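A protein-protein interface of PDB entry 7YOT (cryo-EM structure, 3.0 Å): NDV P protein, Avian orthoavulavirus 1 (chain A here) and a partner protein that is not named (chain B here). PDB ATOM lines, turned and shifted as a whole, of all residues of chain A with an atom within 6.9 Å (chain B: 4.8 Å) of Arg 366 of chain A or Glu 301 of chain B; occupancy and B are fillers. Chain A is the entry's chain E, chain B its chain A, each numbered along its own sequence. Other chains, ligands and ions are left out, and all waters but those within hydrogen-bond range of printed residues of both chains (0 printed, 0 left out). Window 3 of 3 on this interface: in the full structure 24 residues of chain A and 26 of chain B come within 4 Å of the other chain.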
ATOM      1  N   ALA A 361     -31.194 -31.754  -2.426  1.00  0.00           N
ATOM      2  CA  ALA A 361     -29.756 -31.553  -2.557  1.00  0.00           C
ATOM      3  C   ALA A 361     -29.441 -30.418  -3.523  1.00  0.00           C
ATOM      4  O   ALA A 361     -28.470 -29.682  -3.325  1.00  0.00           O
ATOM      5  CB  ALA A 361     -29.083 -32.844  -3.006  1.00  0.00           C
ATOM      6  N   LEU A 362     -30.253 -30.256  -4.569  1.00  0.00           N
ATOM      7  CA  LEU A 362     -30.045 -29.155  -5.505  1.00  0.00           C
ATOM      8  C   LEU A 362     -30.404 -27.811  -4.880  1.00  0.00           C
ATOM      9  O   LEU A 362     -29.733 -26.810  -5.142  1.00  0.00           O
ATOM     10  CB  LEU A 362     -30.843 -29.364  -6.796  1.00  0.00           C
ATOM     11  CG  LEU A 362     -30.247 -30.076  -8.025  1.00  0.00           C
ATOM     12  CD1 LEU A 362     -28.907 -29.495  -8.373  1.00  0.00           C
ATOM     13  CD2 LEU A 362     -30.138 -31.569  -7.977  1.00  0.00           C
ATOM     14  N   ILE A 363     -31.454 -27.758  -4.055  1.00  0.00           N
ATOM     15  CA  ILE A 363     -31.808 -26.492  -3.413  1.00  0.00           C
ATOM     16  C   ILE A 363     -30.802 -26.136  -2.321  1.00  0.00           C
ATOM     17  O   ILE A 363     -30.384 -24.979  -2.198  1.00  0.00           O
ATOM     18  CB  ILE A 363     -33.252 -26.550  -2.877  1.00  0.00           C
ATOM     19  CG1 ILE A 363     -34.243 -26.652  -4.032  1.00  0.00           C
ATOM     20  CG2 ILE A 363     -33.593 -25.321  -2.067  1.00  0.00           C
ATOM     21  CD1 ILE A 363     -35.644 -26.997  -3.590  1.00  0.00           C
ATOM     22  N   LEU A 364     -30.364 -27.127  -1.537  1.00  0.00           N
ATOM     23  CA  LEU A 364     -29.466 -26.855  -0.418  1.00  0.00           C
ATOM     24  C   LEU A 364     -28.046 -26.517  -0.858  1.00  0.00           C
ATOM     25  O   LEU A 364     -27.400 -25.669  -0.235  1.00  0.00           O
ATOM     26  CB  LEU A 364     -29.440 -28.047   0.538  1.00  0.00           C
ATOM     27  CG  LEU A 364     -30.371 -28.056   1.752  1.00  0.00           C
ATOM     28  CD1 LEU A 364     -31.822 -28.088   1.386  1.00  0.00           C
ATOM     29  CD2 LEU A 364     -30.035 -29.265   2.599  1.00  0.00           C
ATOM     30  N   SER A 365     -27.536 -27.150  -1.912  1.00  0.00           N
ATOM     31  CA  SER A 365     -26.117 -27.039  -2.224  1.00  0.00           C
ATOM     32  C   SER A 365     -25.781 -25.996  -3.282  1.00  0.00           C
ATOM     33  O   SER A 365     -24.625 -25.573  -3.352  1.00  0.00           O
ATOM     34  CB  SER A 365     -25.568 -28.394  -2.674  1.00  0.00           C
ATOM     35  OG  SER A 365     -26.174 -28.798  -3.881  1.00  0.00           O
ATOM     36  N   ARG A 366     -26.734 -25.576  -4.102  1.00  0.00           N
ATOM     37  CA  ARG A 366     -26.408 -24.572  -5.103  1.00  0.00           C
ATOM     38  C   ARG A 366     -26.434 -23.179  -4.492  1.00  0.00           C
ATOM     39  O   ARG A 366     -27.094 -22.951  -3.474  1.00  0.00           O
ATOM     40  CB  ARG A 366     -27.388 -24.648  -6.271  1.00  0.00           C
ATOM     41  CG  ARG A 366     -27.265 -25.900  -7.108  1.00  0.00           C
ATOM     42  CD  ARG A 366     -28.266 -25.899  -8.240  1.00  0.00           C
ATOM     43  NE  ARG A 366     -27.940 -24.949  -9.293  1.00  0.00           N
ATOM     44  CZ  ARG A 366     -27.210 -25.246 -10.361  1.00  0.00           C
ATOM     45  NH1 ARG A 366     -26.727 -26.467 -10.517  1.00  0.00           N
ATOM     46  NH2 ARG A 366     -26.963 -24.321 -11.275  1.00  0.00           N
ATOM     47  N   PRO A 367     -25.700 -22.226  -5.074  1.00  0.00           N
ATOM     48  CA  PRO A 367     -25.813 -20.831  -4.625  1.00  0.00           C
ATOM     49  C   PRO A 367     -27.187 -20.263  -4.944  1.00  0.00           C
ATOM     50  O   PRO A 367     -27.661 -20.350  -6.078  1.00  0.00           O
ATOM     51  CB  PRO A 367     -24.713 -20.112  -5.415  1.00  0.00           C
ATOM     52  CG  PRO A 367     -23.745 -21.174  -5.754  1.00  0.00           C
ATOM     53  CD  PRO A 367     -24.558 -22.405  -5.987  1.00  0.00           C
ATOM     54  N   MET A 368     -27.817 -19.673  -3.932  1.00  0.00           N
ATOM     55  CA  MET A 368     -29.196 -19.223  -4.039  1.00  0.00           C
ATOM     56  C   MET A 368     -29.447 -18.217  -2.927  1.00  0.00           C
ATOM     57  O   MET A 368     -28.817 -18.281  -1.868  1.00  0.00           O
ATOM     58  CB  MET A 368     -30.157 -20.415  -3.943  1.00  0.00           C
ATOM     59  CG  MET A 368     -31.588 -20.151  -4.351  1.00  0.00           C
ATOM     60  SD  MET A 368     -32.571 -21.654  -4.245  1.00  0.00           S
ATOM     61  CE  MET A 368     -31.853 -22.612  -5.572  1.00  0.00           C
ATOM     62  N   HIS A 369     -30.351 -17.279  -3.184  1.00  0.00           N
ATOM     63  CA  HIS A 369     -30.704 -16.287  -2.176  1.00  0.00           C
ATOM     64  C   HIS A 369     -31.463 -16.975  -1.043  1.00  0.00           C
ATOM     65  O   HIS A 369     -32.323 -17.823  -1.312  1.00  0.00           O
ATOM     66  CB  HIS A 369     -31.539 -15.174  -2.807  1.00  0.00           C
ATOM     67  CG  HIS A 369     -31.782 -14.007  -1.903  1.00  0.00           C
ATOM     68  ND1 HIS A 369     -30.787 -13.122  -1.549  1.00  0.00           N
ATOM     69  CD2 HIS A 369     -32.910 -13.564  -1.299  1.00  0.00           C
ATOM     70  CE1 HIS A 369     -31.288 -12.193  -0.754  1.00  0.00           C
ATOM     71  NE2 HIS A 369     -32.576 -12.437  -0.589  1.00  0.00           N
ATOM     72  N   SER A 373     -34.389 -19.882  -1.257  1.00  0.00           N
ATOM     73  CA  SER A 373     -34.112 -21.279  -0.932  1.00  0.00           C
ATOM     74  C   SER A 373     -35.108 -21.812   0.089  1.00  0.00           C
ATOM     75  O   SER A 373     -35.580 -22.950  -0.030  1.00  0.00           O
ATOM     76  CB  SER A 373     -32.684 -21.430  -0.415  1.00  0.00           C
ATOM     77  OG  SER A 373     -32.531 -20.806   0.846  1.00  0.00           O
ATOM     78  N   ALA A 396     -35.567 -24.578  -9.848  1.00  0.00           N
ATOM     79  CA  ALA A 396     -34.349 -24.310  -9.090  1.00  0.00           C
ATOM     80  C   ALA A 396     -33.123 -24.191  -9.983  1.00  0.00           C
ATOM     81  O   ALA A 396     -32.295 -23.299  -9.780  1.00  0.00           O
ATOM     82  CB  ALA A 396     -34.110 -25.412  -8.056  1.00  0.00           C
ATOM     83  N   LEU A 397     -32.988 -25.081 -10.969  1.00  0.00           N
ATOM     84  CA  LEU A 397     -31.842 -25.039 -11.868  1.00  0.00           C
ATOM     85  C   LEU A 397     -31.906 -23.868 -12.835  1.00  0.00           C
ATOM     86  O   LEU A 397     -30.874 -23.485 -13.394  1.00  0.00           O
ATOM     87  CB  LEU A 397     -31.738 -26.349 -12.641  1.00  0.00           C
ATOM     88  CG  LEU A 397     -31.386 -27.547 -11.766  1.00  0.00           C
ATOM     89  CD1 LEU A 397     -31.481 -28.840 -12.541  1.00  0.00           C
ATOM     90  CD2 LEU A 397     -30.002 -27.366 -11.212  1.00  0.00           C
ATOM     91  N   ASN A 398     -33.090 -23.293 -13.041  1.00  0.00           N
ATOM     92  CA  ASN A 398     -33.264 -22.103 -13.861  1.00  0.00           C
ATOM     93  C   ASN A 398     -33.340 -20.841 -13.014  1.00  0.00           C
ATOM     94  O   ASN A 398     -34.074 -19.907 -13.349  1.00  0.00           O
ATOM     95  CB  ASN A 398     -34.514 -22.241 -14.727  1.00  0.00           C
ATOM     96  CG  ASN A 398     -34.382 -23.336 -15.763  1.00  0.00           C
ATOM     97  OD1 ASN A 398     -33.333 -23.495 -16.384  1.00  0.00           O
ATOM     98  ND2 ASN A 398     -35.448 -24.102 -15.951  1.00  0.00           N
ATOM     99  N   GLY A 399     -32.598 -20.803 -11.913  1.00  0.00           N
ATOM    100  CA  GLY A 399     -32.627 -19.676 -11.003  1.00  0.00           C
ATOM    101  C   GLY A 399     -32.814 -20.111  -9.563  1.00  0.00           C
ATOM    102  O   GLY A 399     -32.754 -19.293  -8.645  1.00  0.00           O
ATOM    103  N   VAL B 297     -20.317 -32.986  -5.952  1.00  0.00           N
ATOM    104  CA  VAL B 297     -19.600 -31.974  -6.715  1.00  0.00           C
ATOM    105  C   VAL B 297     -20.399 -31.594  -7.954  1.00  0.00           C
ATOM    106  O   VAL B 297     -20.441 -30.427  -8.354  1.00  0.00           O
ATOM    107  CB  VAL B 297     -18.193 -32.485  -7.075  1.00  0.00           C
ATOM    108  CG1 VAL B 297     -17.402 -31.443  -7.833  1.00  0.00           C
ATOM    109  CG2 VAL B 297     -17.453 -32.895  -5.842  1.00  0.00           C
ATOM    110  N   GLN B 298     -21.075 -32.564  -8.557  1.00  0.00           N
ATOM    111  CA  GLN B 298     -21.856 -32.333  -9.761  1.00  0.00           C
ATOM    112  C   GLN B 298     -23.204 -31.686  -9.454  1.00  0.00           C
ATOM    113  O   GLN B 298     -23.953 -31.367 -10.375  1.00  0.00           O
ATOM    114  CB  GLN B 298     -22.041 -33.663 -10.497  1.00  0.00           C
ATOM    115  CG  GLN B 298     -22.337 -33.578 -11.975  1.00  0.00           C
ATOM    116  CD  GLN B 298     -22.629 -34.924 -12.569  1.00  0.00           C
ATOM    117  OE1 GLN B 298     -22.711 -35.912 -11.856  1.00  0.00           O
ATOM    118  NE2 GLN B 298     -22.791 -34.977 -13.880  1.00  0.00           N
ATOM    119  N   LEU B 299     -23.537 -31.471  -8.183  1.00  0.00           N
ATOM    120  CA  LEU B 299     -24.680 -30.626  -7.865  1.00  0.00           C
ATOM    121  C   LEU B 299     -24.412 -29.176  -8.240  1.00  0.00           C
ATOM    122  O   LEU B 299     -25.349 -28.419  -8.503  1.00  0.00           O
ATOM    123  CB  LEU B 299     -25.013 -30.728  -6.377  1.00  0.00           C
ATOM    124  CG  LEU B 299     -25.480 -32.074  -5.825  1.00  0.00           C
ATOM    125  CD1 LEU B 299     -25.602 -32.032  -4.329  1.00  0.00           C
ATOM    126  CD2 LEU B 299     -26.796 -32.473  -6.429  1.00  0.00           C
ATOM    127  N   LEU B 300     -23.147 -28.775  -8.259  1.00  0.00           N
ATOM    128  CA  LEU B 300     -22.750 -27.386  -8.480  1.00  0.00           C
ATOM    129  C   LEU B 300     -22.362 -27.154  -9.940  1.00  0.00           C
ATOM    130  O   LEU B 300     -21.269 -26.696 -10.249  1.00  0.00           O
ATOM    131  CB  LEU B 300     -21.600 -27.011  -7.550  1.00  0.00           C
ATOM    132  CG  LEU B 300     -21.843 -26.730  -6.067  1.00  0.00           C
ATOM    133  CD1 LEU B 300     -21.989 -27.987  -5.243  1.00  0.00           C
ATOM    134  CD2 LEU B 300     -20.726 -25.882  -5.520  1.00  0.00           C
ATOM    135  N   GLU B 301     -23.257 -27.455 -10.813  1.00  0.00           N
ATOM    136  CA  GLU B 301     -23.041 -27.248 -12.236  1.00  0.00           C
ATOM    137  C   GLU B 301     -23.405 -25.823 -12.639  1.00  0.00           C
ATOM    138  O   GLU B 301     -24.225 -25.178 -11.981  1.00  0.00           O
ATOM    139  CB  GLU B 301     -23.874 -28.234 -13.046  1.00  0.00           C
ATOM    140  CG  GLU B 301     -23.345 -29.648 -13.038  1.00  0.00           C
ATOM    141  CD  GLU B 301     -22.077 -29.810 -13.837  1.00  0.00           C
ATOM    142  OE1 GLU B 301     -21.911 -29.089 -14.837  1.00  0.00           O
ATOM    143  OE2 GLU B 301     -21.252 -30.667 -13.477  1.00  0.00           O
ATOM    144  N   PRO B 302     -22.795 -25.289 -13.702  1.00  0.00           N
ATOM    145  CA  PRO B 302     -23.215 -23.966 -14.177  1.00  0.00           C
ATOM    146  C   PRO B 302     -24.556 -23.982 -14.882  1.00  0.00           C
ATOM    147  O   PRO B 302     -25.291 -22.991 -14.817  1.00  0.00           O
ATOM    148  CB  PRO B 302     -22.083 -23.564 -15.130  1.00  0.00           C
ATOM    149  CG  PRO B 302     -21.503 -24.843 -15.586  1.00  0.00           C
ATOM    150  CD  PRO B 302     -21.605 -25.771 -14.423  1.00  0.00           C
ATOM    151  N   SER B 303     -24.896 -25.071 -15.553  1.00  0.00           N
ATOM    152  CA  SER B 303     -26.148 -25.200 -16.268  1.00  0.00           C
ATOM    153  C   SER B 303     -27.158 -25.961 -15.421  1.00  0.00           C
ATOM    154  O   SER B 303     -26.934 -26.244 -14.244  1.00  0.00           O
ATOM    155  CB  SER B 303     -25.920 -25.909 -17.600  1.00  0.00           C
ATOM    156  OG  SER B 303     -25.086 -25.153 -18.445  1.00  0.00           O
ATOM    157  N   THR B 305     -28.247 -28.856 -16.818  1.00  0.00           N
ATOM    158  CA  THR B 305     -27.929 -30.226 -17.177  1.00  0.00           C
ATOM    159  C   THR B 305     -26.783 -30.728 -16.317  1.00  0.00           C
ATOM    160  O   THR B 305     -26.051 -29.946 -15.706  1.00  0.00           O
ATOM    161  CB  THR B 305     -27.545 -30.353 -18.643  1.00  0.00           C
ATOM    162  OG1 THR B 305     -26.290 -29.715 -18.836  1.00  0.00           O
ATOM    163  CG2 THR B 305     -28.581 -29.683 -19.517  1.00  0.00           C
ATOM    164  N   PHE B 306     -26.694 -32.059 -16.226  1.00  0.00           N
ATOM    165  CA  PHE B 306     -25.724 -32.869 -15.484  1.00  0.00           C
ATOM    166  C   PHE B 306     -25.880 -32.757 -13.971  1.00  0.00           C
ATOM    167  O   PHE B 306     -25.304 -33.562 -13.243  1.00  0.00           O
ATOM    168  CB  PHE B 306     -24.279 -32.525 -15.866  1.00  0.00           C
ATOM    169  CG  PHE B 306     -23.925 -32.846 -17.284  1.00  0.00           C
ATOM    170  CD1 PHE B 306     -24.601 -33.820 -17.991  1.00  0.00           C
ATOM    171  CD2 PHE B 306     -22.945 -32.119 -17.927  1.00  0.00           C
ATOM    172  CE1 PHE B 306     -24.276 -34.086 -19.297  1.00  0.00           C
ATOM    173  CE2 PHE B 306     -22.622 -32.378 -19.230  1.00  0.00           C
ATOM    174  CZ  PHE B 306     -23.285 -33.359 -19.916  1.00  0.00           C
ATOM    175  N   ALA B 307     -26.704 -31.843 -13.479  1.00  0.00           N
ATOM    176  CA  ALA B 307     -26.807 -31.597 -12.051  1.00  0.00           C
ATOM    177  C   ALA B 307     -27.692 -32.653 -11.412  1.00  0.00           C
ATOM    178  O   ALA B 307     -28.860 -32.798 -11.783  1.00  0.00           O
ATOM    179  CB  ALA B 307     -27.366 -30.203 -11.787  1.00  0.00           C
ATOM    180  N   SER B 804     -19.399 -33.976 -16.961  1.00  0.00           N
ATOM    181  CA  SER B 804     -19.497 -32.725 -16.233  1.00  0.00           C
ATOM    182  C   SER B 804     -18.955 -31.588 -17.077  1.00  0.00           C
ATOM    183  O   SER B 804     -18.001 -31.755 -17.834  1.00  0.00           O
ATOM    184  CB  SER B 804     -18.746 -32.801 -14.906  1.00  0.00           C
ATOM    185  OG  SER B 804     -18.908 -31.602 -14.179  1.00  0.00           O
ATOM    186  N   ASP B 805     -19.568 -30.421 -16.930  1.00  0.00           N
ATOM    187  CA  ASP B 805     -19.033 -29.225 -17.561  1.00  0.00           C
ATOM    188  C   ASP B 805     -17.899 -28.606 -16.772  1.00  0.00           C
ATOM    189  O   ASP B 805     -17.269 -27.665 -17.261  1.00  0.00           O
ATOM    190  CB  ASP B 805     -20.122 -28.171 -17.744  1.00  0.00           C
ATOM    191  CG  ASP B 805     -21.078 -28.508 -18.852  1.00  0.00           C
ATOM    192  OD1 ASP B 805     -20.660 -29.190 -19.805  1.00  0.00           O
ATOM    193  OD2 ASP B 805     -22.247 -28.084 -18.779  1.00  0.00           O
ATOM    194  N   THR B 806     -17.629 -29.097 -15.573  1.00  0.00           N
ATOM    195  CA  THR B 806     -16.770 -28.378 -14.652  1.00  0.00           C
ATOM    196  C   THR B 806     -15.540 -29.168 -14.244  1.00  0.00           C
ATOM    197  O   THR B 806     -14.427 -28.640 -14.295  1.00  0.00           O
ATOM    198  CB  THR B 806     -17.574 -27.993 -13.412  1.00  0.00           C
ATOM    199  OG1 THR B 806     -18.789 -27.368 -13.821  1.00  0.00           O
ATOM    200  CG2 THR B 806     -16.824 -26.995 -12.642  1.00  0.00           C
ATOM    201  N   PHE B 807     -15.701 -30.421 -13.844  1.00  0.00           N
ATOM    202  CA  PHE B 807     -14.600 -31.166 -13.269  1.00  0.00           C
ATOM    203  C   PHE B 807     -14.375 -32.464 -14.024  1.00  0.00           C
ATOM    204  O   PHE B 807     -15.233 -32.941 -14.765  1.00  0.00           O
ATOM    205  CB  PHE B 807     -14.841 -31.471 -11.780  1.00  0.00           C
ATOM    206  CG  PHE B 807     -15.931 -32.481 -11.516  1.00  0.00           C
ATOM    207  CD1 PHE B 807     -17.252 -32.088 -11.471  1.00  0.00           C
ATOM    208  CD2 PHE B 807     -15.627 -33.807 -11.246  1.00  0.00           C
ATOM    209  CE1 PHE B 807     -18.243 -33.000 -11.219  1.00  0.00           C
ATOM    210  CE2 PHE B 807     -16.615 -34.718 -10.998  1.00  0.00           C
ATOM    211  CZ  PHE B 807     -17.923 -34.311 -10.975  1.00  0.00           C
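Glu 301 of chain B touches one residue of chain A.
Of the printed residues of chain B, Ala 361 of chain A touches Leu 299.
Printed residues of chain B within 4 Å of Leu 362 of chain A: Leu 299 (3.7 Å) and Ala 307 (3.8 Å).
Printed residues of chain A within 4 Å of Leu 299 of chain B: Ala 361, Leu 362, Ser 365 and Arg 366.
Of the printed residues of chain B, Leu 397 of chain A touches Ala 307 (3.9 Å).
Of the printed residues of chain A, Ala 307 of chain B touches Leu 362, Arg 366 and Leu 397.
Leu 364 of chain A touches none of the printed residues of chain B.
The nearest printed residue of chain A that does not touch Leu 299 of chain B is Leu 397 of chain A (5.5 Å).
Of the 14 printed residues of chain B, 4 touch a printed residue of chain A.
Printed residues of chain B that touch a printed residue of chain A: Leu 299, Glu 301, Ser 303 and Ala 307.
Hydrophobic or aromatic side chains of chain B within 4 Å of the printed part of chain A: Leu 299 and Ala 307.
Along chain A the printed residues that touch a printed residue of chain B span positions 361 to 397.
The backbone carbonyl oxygen (O) of Ala 361 of chain A lies within hydrogen-bond range of the side-chain hydroxyl (OG) of Ser 365 of chain A, at 2.5 Å.
The backbone NH (N) of Asp 805 of chain B is in hydrogen-bond range of the side-chain carboxylate (OE1) of Glu 301 of chain B (3.4 Å).
OE2 of Glu 301 of chain B sits at hydrogen-bond distance from OG of Ser 804 of chain B (2.6 Å).
NH2 of Arg 366 of chain A lies within hydrogen-bond range of O of Glu 301 of chain B (3.0 Å).
O of Leu 299 of chain B lies within hydrogen-bond range of NH1 of Arg 366 of chain A (3.1 Å).
Among the printed residues, merely in contact across the chains: Ala 361 of chain A with Leu 299 of chain B (3.8 Å), Leu 362 of chain A with Leu 299 of chain B (3.7 Å), Leu 362 of chain A with Ala 307 of chain B (3.8 Å), Ser 365 of chain A with Leu 299 of chain B (3.3 Å), Arg 366 of chain A with Ser 303 of chain B (3.5 Å), Arg 366 of chain A with Ala 307 of chain B (3.997 Å) and Leu 397 of chain A with Ala 307 of chain B (3.9 Å).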
